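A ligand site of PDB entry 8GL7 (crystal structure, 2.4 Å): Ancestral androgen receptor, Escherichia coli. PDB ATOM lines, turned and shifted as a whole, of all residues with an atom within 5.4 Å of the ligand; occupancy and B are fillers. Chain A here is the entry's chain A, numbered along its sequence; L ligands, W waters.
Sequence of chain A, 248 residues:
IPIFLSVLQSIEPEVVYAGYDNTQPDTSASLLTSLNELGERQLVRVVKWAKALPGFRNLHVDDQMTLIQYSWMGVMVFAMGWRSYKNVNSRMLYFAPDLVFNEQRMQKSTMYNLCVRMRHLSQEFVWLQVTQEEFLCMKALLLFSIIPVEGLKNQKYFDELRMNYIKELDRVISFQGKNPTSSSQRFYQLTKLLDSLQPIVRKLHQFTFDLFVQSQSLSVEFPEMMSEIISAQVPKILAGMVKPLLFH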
ATOM      1  N   LEU A  32      19.479  31.943 -13.793  1.00  0.00           N
ATOM      2  CA  LEU A  32      19.182  30.532 -13.565  1.00  0.00           C
ATOM      3  C   LEU A  32      19.595  29.685 -14.769  1.00  0.00           C
ATOM      4  O   LEU A  32      20.075  28.566 -14.599  1.00  0.00           O
ATOM      5  CB  LEU A  32      17.691  30.353 -13.249  1.00  0.00           C
ATOM      6  CG  LEU A  32      17.229  31.060 -11.978  1.00  0.00           C
ATOM      7  CD1 LEU A  32      15.741  30.956 -11.748  1.00  0.00           C
ATOM      8  CD2 LEU A  32      17.967  30.529 -10.807  1.00  0.00           C
ATOM      9  N   LEU A  35      23.318  29.222 -14.563  1.00  0.00           N
ATOM     10  CA  LEU A  35      23.586  28.204 -13.558  1.00  0.00           C
ATOM     11  C   LEU A  35      23.314  26.794 -14.073  1.00  0.00           C
ATOM     12  O   LEU A  35      24.093  25.878 -13.793  1.00  0.00           O
ATOM     13  CB  LEU A  35      22.747  28.507 -12.302  1.00  0.00           C
ATOM     14  CG  LEU A  35      23.218  29.620 -11.390  1.00  0.00           C
ATOM     15  CD1 LEU A  35      22.205  29.803 -10.232  1.00  0.00           C
ATOM     16  CD2 LEU A  35      24.626  29.381 -10.804  1.00  0.00           C
ATOM     17  N   ASN A  36      22.214  26.591 -14.796  1.00  0.00           N
ATOM     18  CA  ASN A  36      21.938  25.286 -15.370  1.00  0.00           C
ATOM     19  C   ASN A  36      23.041  24.823 -16.329  1.00  0.00           C
ATOM     20  O   ASN A  36      23.440  23.652 -16.299  1.00  0.00           O
ATOM     21  CB  ASN A  36      20.602  25.304 -16.107  1.00  0.00           C
ATOM     22  CG  ASN A  36      19.449  25.287 -15.152  1.00  0.00           C
ATOM     23  OD1 ASN A  36      19.586  24.892 -13.967  1.00  0.00           O
ATOM     24  ND2 ASN A  36      18.298  25.756 -15.616  1.00  0.00           N
ATOM     25  N   LEU A  38      26.329  25.833 -16.461  1.00  0.00           N
ATOM     26  CA  LEU A  38      27.437  25.494 -15.567  1.00  0.00           C
ATOM     27  C   LEU A  38      27.218  24.151 -14.880  1.00  0.00           C
ATOM     28  O   LEU A  38      28.114  23.307 -14.856  1.00  0.00           O
ATOM     29  CB  LEU A  38      27.597  26.616 -14.531  1.00  0.00           C
ATOM     30  CG  LEU A  38      28.590  26.436 -13.404  1.00  0.00           C
ATOM     31  CD1 LEU A  38      30.005  26.340 -13.965  1.00  0.00           C
ATOM     32  CD2 LEU A  38      28.497  27.602 -12.376  1.00  0.00           C
ATOM     33  N   GLY A  39      26.012  23.930 -14.334  1.00  0.00           N
ATOM     34  CA  GLY A  39      25.683  22.643 -13.729  1.00  0.00           C
ATOM     35  C   GLY A  39      25.878  21.451 -14.648  1.00  0.00           C
ATOM     36  O   GLY A  39      26.401  20.414 -14.221  1.00  0.00           O
ATOM     37  N   GLN A  42      29.709  20.952 -15.100  1.00  0.00           N
ATOM     38  CA  GLN A  42      30.270  20.413 -13.881  1.00  0.00           C
ATOM     39  C   GLN A  42      29.857  18.955 -13.683  1.00  0.00           C
ATOM     40  O   GLN A  42      30.649  18.150 -13.198  1.00  0.00           O
ATOM     41  CB  GLN A  42      29.801  21.178 -12.640  1.00  0.00           C
ATOM     42  CG  GLN A  42      30.061  22.649 -12.591  1.00  0.00           C
ATOM     43  CD  GLN A  42      30.012  23.159 -11.160  1.00  0.00           C
ATOM     44  OE1 GLN A  42      29.682  22.416 -10.230  1.00  0.00           O
ATOM     45  NE2 GLN A  42      30.320  24.434 -10.971  1.00  0.00           N
ATOM     46  N   TRP A  72      24.769  14.555  -6.823  1.00  0.00           N
ATOM     47  CA  TRP A  72      25.411  15.614  -7.606  1.00  0.00           C
ATOM     48  C   TRP A  72      25.163  16.988  -6.979  1.00  0.00           C
ATOM     49  O   TRP A  72      26.090  17.815  -6.906  1.00  0.00           O
ATOM     50  CB  TRP A  72      24.904  15.573  -9.061  1.00  0.00           C
ATOM     51  CG  TRP A  72      23.469  15.892  -9.273  1.00  0.00           C
ATOM     52  CD1 TRP A  72      22.432  14.992  -9.341  1.00  0.00           C
ATOM     53  CD2 TRP A  72      22.894  17.183  -9.477  1.00  0.00           C
ATOM     54  NE1 TRP A  72      21.249  15.665  -9.545  1.00  0.00           N
ATOM     55  CE2 TRP A  72      21.510  17.006  -9.628  1.00  0.00           C
ATOM     56  CE3 TRP A  72      23.423  18.481  -9.523  1.00  0.00           C
ATOM     57  CZ2 TRP A  72      20.625  18.081  -9.832  1.00  0.00           C
ATOM     58  CZ3 TRP A  72      22.561  19.546  -9.699  1.00  0.00           C
ATOM     59  CH2 TRP A  72      21.166  19.347  -9.865  1.00  0.00           C
ATOM     60  N   MET A  73      23.967  17.234  -6.448  1.00  0.00           N
ATOM     61  CA  MET A  73      23.657  18.539  -5.869  1.00  0.00           C
ATOM     62  C   MET A  73      24.530  18.808  -4.644  1.00  0.00           C
ATOM     63  O   MET A  73      25.082  19.903  -4.482  1.00  0.00           O
ATOM     64  CB  MET A  73      22.181  18.597  -5.495  1.00  0.00           C
ATOM     65  CG  MET A  73      21.753  19.844  -4.777  1.00  0.00           C
ATOM     66  SD  MET A  73      21.811  21.344  -5.864  1.00  0.00           S
ATOM     67  CE  MET A  73      20.374  21.132  -6.828  1.00  0.00           C
ATOM     68  N   MET A  76      28.203  19.429  -5.644  1.00  0.00           N
ATOM     69  CA  MET A  76      28.448  20.684  -6.309  1.00  0.00           C
ATOM     70  C   MET A  76      28.296  21.861  -5.354  1.00  0.00           C
ATOM     71  O   MET A  76      29.074  22.809  -5.418  1.00  0.00           O
ATOM     72  CB  MET A  76      27.511  20.832  -7.493  1.00  0.00           C
ATOM     73  CG  MET A  76      27.973  20.079  -8.735  1.00  0.00           C
ATOM     74  SD  MET A  76      26.717  20.119 -10.021  1.00  0.00           S
ATOM     75  CE  MET A  76      27.049  18.575 -10.841  1.00  0.00           C
ATOM     76  N   VAL A  77      27.314  21.808  -4.459  1.00  0.00           N
ATOM     77  CA  VAL A  77      27.179  22.855  -3.442  1.00  0.00           C
ATOM     78  C   VAL A  77      28.429  22.901  -2.555  1.00  0.00           C
ATOM     79  O   VAL A  77      28.937  23.987  -2.226  1.00  0.00           O
ATOM     80  CB  VAL A  77      25.914  22.652  -2.597  1.00  0.00           C
ATOM     81  CG1 VAL A  77      25.919  23.590  -1.454  1.00  0.00           C
ATOM     82  CG2 VAL A  77      24.680  22.857  -3.451  1.00  0.00           C
ATOM     83  N   MET A  80      31.319  24.372  -4.453  1.00  0.00           N
ATOM     84  CA  MET A  80      31.132  25.798  -4.668  1.00  0.00           C
ATOM     85  C   MET A  80      31.414  26.587  -3.388  1.00  0.00           C
ATOM     86  O   MET A  80      32.015  27.660  -3.428  1.00  0.00           O
ATOM     87  CB  MET A  80      29.698  26.048  -5.157  1.00  0.00           C
ATOM     88  CG  MET A  80      29.368  27.462  -5.599  1.00  0.00           C
ATOM     89  SD  MET A  80      28.917  28.450  -4.175  1.00  0.00           S
ATOM     90  CE  MET A  80      27.281  27.718  -3.758  1.00  0.00           C
ATOM     91  N   ARG A  83      35.073  26.866  -3.180  1.00  0.00           N
ATOM     92  CA  ARG A  83      35.591  27.892  -4.077  1.00  0.00           C
ATOM     93  C   ARG A  83      35.345  29.294  -3.507  1.00  0.00           C
ATOM     94  O   ARG A  83      36.214  30.174  -3.598  1.00  0.00           O
ATOM     95  CB  ARG A  83      34.952  27.811  -5.466  1.00  0.00           C
ATOM     96  CG  ARG A  83      35.415  26.653  -6.301  1.00  0.00           C
ATOM     97  CD  ARG A  83      35.016  26.872  -7.785  1.00  0.00           C
ATOM     98  NE  ARG A  83      33.566  26.929  -7.987  1.00  0.00           N
ATOM     99  CZ  ARG A  83      32.765  25.877  -7.982  1.00  0.00           C
ATOM    100  NH1 ARG A  83      33.237  24.661  -7.781  1.00  0.00           N
ATOM    101  NH2 ARG A  83      31.459  26.046  -8.203  1.00  0.00           N
ATOM    102  N   PHE A  95      30.198  30.754  -8.035  1.00  0.00           N
ATOM    103  CA  PHE A  95      29.745  29.618  -8.843  1.00  0.00           C
ATOM    104  C   PHE A  95      30.791  29.232  -9.867  1.00  0.00           C
ATOM    105  O   PHE A  95      31.063  28.046 -10.098  1.00  0.00           O
ATOM    106  CB  PHE A  95      28.412  29.948  -9.493  1.00  0.00           C
ATOM    107  CG  PHE A  95      27.289  29.922  -8.533  1.00  0.00           C
ATOM    108  CD1 PHE A  95      26.730  28.738  -8.148  1.00  0.00           C
ATOM    109  CD2 PHE A  95      26.770  31.108  -8.003  1.00  0.00           C
ATOM    110  CE1 PHE A  95      25.675  28.712  -7.233  1.00  0.00           C
ATOM    111  CE2 PHE A  95      25.717  31.098  -7.111  1.00  0.00           C
ATOM    112  CZ  PHE A  95      25.177  29.907  -6.730  1.00  0.00           C
ATOM    113  N   MET A 111      16.185  33.112  -5.837  1.00  0.00           N
ATOM    114  CA  MET A 111      16.480  32.082  -4.847  1.00  0.00           C
ATOM    115  C   MET A 111      17.363  32.667  -3.724  1.00  0.00           C
ATOM    116  O   MET A 111      18.348  32.062  -3.275  1.00  0.00           O
ATOM    117  CB  MET A 111      17.146  30.830  -5.457  1.00  0.00           C
ATOM    118  CG  MET A 111      18.333  31.059  -6.385  1.00  0.00           C
ATOM    119  SD  MET A 111      19.274  29.527  -6.782  1.00  0.00           S
ATOM    120  CE  MET A 111      19.670  28.952  -5.128  1.00  0.00           C
ATOM    121  N   MET A 118      23.576  29.066   1.583  1.00  0.00           N
ATOM    122  CA  MET A 118      24.784  28.472   1.010  1.00  0.00           C
ATOM    123  C   MET A 118      26.009  29.322   1.329  1.00  0.00           C
ATOM    124  O   MET A 118      27.108  28.773   1.538  1.00  0.00           O
ATOM    125  CB  MET A 118      24.635  28.323  -0.519  1.00  0.00           C
ATOM    126  CG  MET A 118      23.901  27.063  -0.966  1.00  0.00           C
ATOM    127  SD  MET A 118      23.695  26.974  -2.754  1.00  0.00           S
ATOM    128  CE  MET A 118      22.935  28.582  -3.082  1.00  0.00           C
ATOM    129  N   LEU A 204      17.209  22.847  -1.893  1.00  0.00           N
ATOM    130  CA  LEU A 204      17.646  23.092  -3.261  1.00  0.00           C
ATOM    131  C   LEU A 204      16.944  22.135  -4.228  1.00  0.00           C
ATOM    132  O   LEU A 204      16.614  22.529  -5.353  1.00  0.00           O
ATOM    133  CB  LEU A 204      19.162  22.918  -3.363  1.00  0.00           C
ATOM    134  CG  LEU A 204      20.019  24.000  -2.741  1.00  0.00           C
ATOM    135  CD1 LEU A 204      21.494  23.605  -2.741  1.00  0.00           C
ATOM    136  CD2 LEU A 204      19.835  25.320  -3.507  1.00  0.00           C
ATOM    137  N   PHE A 207      13.492  23.586  -4.796  1.00  0.00           N
ATOM    138  CA  PHE A 207      13.552  24.718  -5.712  1.00  0.00           C
ATOM    139  C   PHE A 207      13.797  24.245  -7.137  1.00  0.00           C
ATOM    140  O   PHE A 207      13.147  24.720  -8.078  1.00  0.00           O
ATOM    141  CB  PHE A 207      14.668  25.670  -5.286  1.00  0.00           C
ATOM    142  CG  PHE A 207      14.640  26.988  -6.000  1.00  0.00           C
ATOM    143  CD1 PHE A 207      13.833  28.001  -5.576  1.00  0.00           C
ATOM    144  CD2 PHE A 207      15.454  27.194  -7.096  1.00  0.00           C
ATOM    145  CE1 PHE A 207      13.809  29.226  -6.264  1.00  0.00           C
ATOM    146  CE2 PHE A 207      15.435  28.400  -7.771  1.00  0.00           C
ATOM    147  CZ  PHE A 207      14.603  29.406  -7.362  1.00  0.00           C
ATOM    148  N   THR A 208      14.788  23.361  -7.332  1.00  0.00           N
ATOM    149  CA  THR A 208      15.046  22.753  -8.632  1.00  0.00           C
ATOM    150  C   THR A 208      13.761  22.185  -9.239  1.00  0.00           C
ATOM    151  O   THR A 208      13.449  22.460 -10.388  1.00  0.00           O
ATOM    152  CB  THR A 208      16.097  21.657  -8.478  1.00  0.00           C
ATOM    153  OG1 THR A 208      17.296  22.202  -7.900  1.00  0.00           O
ATOM    154  CG2 THR A 208      16.436  21.030  -9.842  1.00  0.00           C
ATOM    155  N   LEU A 211      11.415  24.893 -10.422  1.00  0.00           N
ATOM    156  CA  LEU A 211      11.899  25.550 -11.637  1.00  0.00           C
ATOM    157  C   LEU A 211      11.712  24.640 -12.852  1.00  0.00           C
ATOM    158  O   LEU A 211      11.291  25.088 -13.917  1.00  0.00           O
ATOM    159  CB  LEU A 211      13.369  25.882 -11.490  1.00  0.00           C
ATOM    160  CG  LEU A 211      13.663  27.347 -11.333  1.00  0.00           C
ATOM    161  CD1 LEU A 211      13.177  27.755  -9.950  1.00  0.00           C
ATOM    162  CD2 LEU A 211      15.133  27.629 -11.519  1.00  0.00           C
ATOM    163  N   VAL A 220      13.577  29.352 -18.416  1.00  0.00           N
ATOM    164  CA  VAL A 220      14.814  28.808 -17.842  1.00  0.00           C
ATOM    165  C   VAL A 220      15.037  27.466 -18.501  1.00  0.00           C
ATOM    166  O   VAL A 220      14.366  26.494 -18.144  1.00  0.00           O
ATOM    167  CB  VAL A 220      14.729  28.685 -16.319  1.00  0.00           C
ATOM    168  CG1 VAL A 220      15.923  27.907 -15.787  1.00  0.00           C
ATOM    169  CG2 VAL A 220      14.653  30.066 -15.708  1.00  0.00           C
ATOM    170  N   PHE A 222      16.737  23.969 -19.054  1.00  0.00           N
ATOM    171  CA  PHE A 222      17.584  22.944 -18.478  1.00  0.00           C
ATOM    172  C   PHE A 222      18.277  22.147 -19.562  1.00  0.00           C
ATOM    173  O   PHE A 222      17.592  21.566 -20.424  1.00  0.00           O
ATOM    174  CB  PHE A 222      16.737  22.025 -17.606  1.00  0.00           C
ATOM    175  CG  PHE A 222      16.335  22.646 -16.301  1.00  0.00           C
ATOM    176  CD1 PHE A 222      15.298  23.550 -16.256  1.00  0.00           C
ATOM    177  CD2 PHE A 222      17.008  22.335 -15.147  1.00  0.00           C
ATOM    178  CE1 PHE A 222      14.937  24.120 -15.064  1.00  0.00           C
ATOM    179  CE2 PHE A 222      16.645  22.903 -13.964  1.00  0.00           C
ATOM    180  CZ  PHE A 222      15.608  23.807 -13.919  1.00  0.00           C
ATOM    181  N   MET A 226      21.087  17.334 -17.256  1.00  0.00           N
ATOM    182  CA  MET A 226      20.428  17.814 -16.059  1.00  0.00           C
ATOM    183  C   MET A 226      18.936  17.489 -16.078  1.00  0.00           C
ATOM    184  O   MET A 226      18.384  17.035 -15.083  1.00  0.00           O
ATOM    185  CB  MET A 226      20.646  19.317 -15.935  1.00  0.00           C
ATOM    186  CG  MET A 226      21.730  19.707 -14.952  1.00  0.00           C
ATOM    187  SD  MET A 226      21.582  21.465 -14.562  1.00  0.00           S
ATOM    188  CE  MET A 226      20.521  21.422 -13.113  1.00  0.00           C
HETATM  189  C1  LIG L   1      25.420  24.892 -10.501  1.00  0.00           C
HETATM  190  C2  LIG L   1      26.894  24.568 -10.307  1.00  0.00           C
HETATM  191  C3  LIG L   1      27.394  25.068  -8.966  1.00  0.00           C
HETATM  192  O1  LIG L   1      28.534  25.455  -8.793  1.00  0.00           O
HETATM  193  C4  LIG L   1      26.427  25.037  -7.871  1.00  0.00           C
HETATM  194  C5  LIG L   1      25.139  24.743  -8.031  1.00  0.00           C
HETATM  195  C6  LIG L   1      24.286  24.540  -6.834  1.00  0.00           C
HETATM  196  C7  LIG L   1      22.895  25.136  -6.961  1.00  0.00           C
HETATM  197  C8  LIG L   1      22.248  24.723  -8.267  1.00  0.00           C
HETATM  198  C9  LIG L   1      23.131  25.051  -9.482  1.00  0.00           C
HETATM  199  C10 LIG L   1      24.522  24.391  -9.354  1.00  0.00           C
HETATM  200  C11 LIG L   1      22.428  24.766 -10.821  1.00  0.00           C
HETATM  201  C12 LIG L   1      21.050  25.426 -10.931  1.00  0.00           C
HETATM  202  C13 LIG L   1      20.186  25.122  -9.724  1.00  0.00           C
HETATM  203  C14 LIG L   1      20.936  25.469  -8.427  1.00  0.00           C
HETATM  204  C15 LIG L   1      19.892  25.342  -7.340  1.00  0.00           C
HETATM  205  C16 LIG L   1      18.576  25.772  -8.042  1.00  0.00           C
HETATM  206  C17 LIG L   1      18.953  26.060  -9.489  1.00  0.00           C
HETATM  207  C18 LIG L   1      19.796  23.666  -9.749  1.00  0.00           C
HETATM  208  C19 LIG L   1      24.395  22.864  -9.378  1.00  0.00           C
HETATM  209  C20 LIG L   1      17.877  25.901 -10.526  1.00  0.00           C
HETATM  210  O2  LIG L   1      17.912  26.371 -11.668  1.00  0.00           O
HETATM  211  C21 LIG L   1      16.675  25.141 -10.068  1.00  0.00           C
HETATM  212  O   HOH W   1      30.406  23.148  -7.713  1.00  0.00           O
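NH2 of Arg 83 is in hydrogen-bond range of O of Phe 95 (2.8 Å). The side-chain hydroxyl of Thr 208 lies within hydrogen-bond range of the backbone carbonyl oxygen of Leu 204 (2.7 Å). The side-chain amide oxygen of Gln 42 lies close to the side-chain sulfur of Met 76 (3.8 Å). NH2 of Arg 83 lies close to NE2 of Gln 42 (3.4 Å). ND2 of Asn 36 lies close to O of Leu 32.
O2 of the ligand sits close to OD1 of Asn 36 (3.2 Å). The side-chain amide nitrogen of Gln 42 sits at hydrogen-bond distance from an oxygen (O1) of the ligand (3.0 Å). An oxygen (O1) of the ligand is in hydrogen-bond range of the guanidinium group of Arg 83, at 3.0 Å.
Leu 35 touches the ligand. Leu 38 touches the ligand (CG to C2, 3.99 Å). Gly 39 touches the ligand (CA to C1, 3.9 Å). Trp 72 touches the ligand (CZ3 to C19, 3.8 Å). Met 73 touches the ligand. Met 76 touches the ligand. CG2 of Val 77 touches C6 of the ligand, 3.8 Å away. CG of Met 80 touches O1 of the ligand (3.9 Å). Phe 95 touches the ligand. CD2 of Leu 204 touches C15 of the ligand (3.8 Å). CD2 of Phe 207 touches C16 of the ligand, at 3.6 Å. Thr 208 touches the ligand (CA to C21, 3.2 Å). Leu 211 touches the ligand (CD2 to O2, 3.1 Å). Hydrophobic or aromatic side chains that line the ligand: Leu 35, Leu 38, Trp 72, Met 73, Met 76, Val 77, Met 80, Phe 95, Leu 204, Phe 207 and Leu 211. Within 4 Å of the ligand: Leu 35, Asn 36, Leu 38, Gly 39, Gln 42, Trp 72, Met 73, Met 76, Val 77, Met 80, Arg 83, Phe 95, Leu 204, Phe 207, Thr 208 and Leu 211. The nearest printed residue that does not touch the ligand is Met 111 (4.02 Å).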
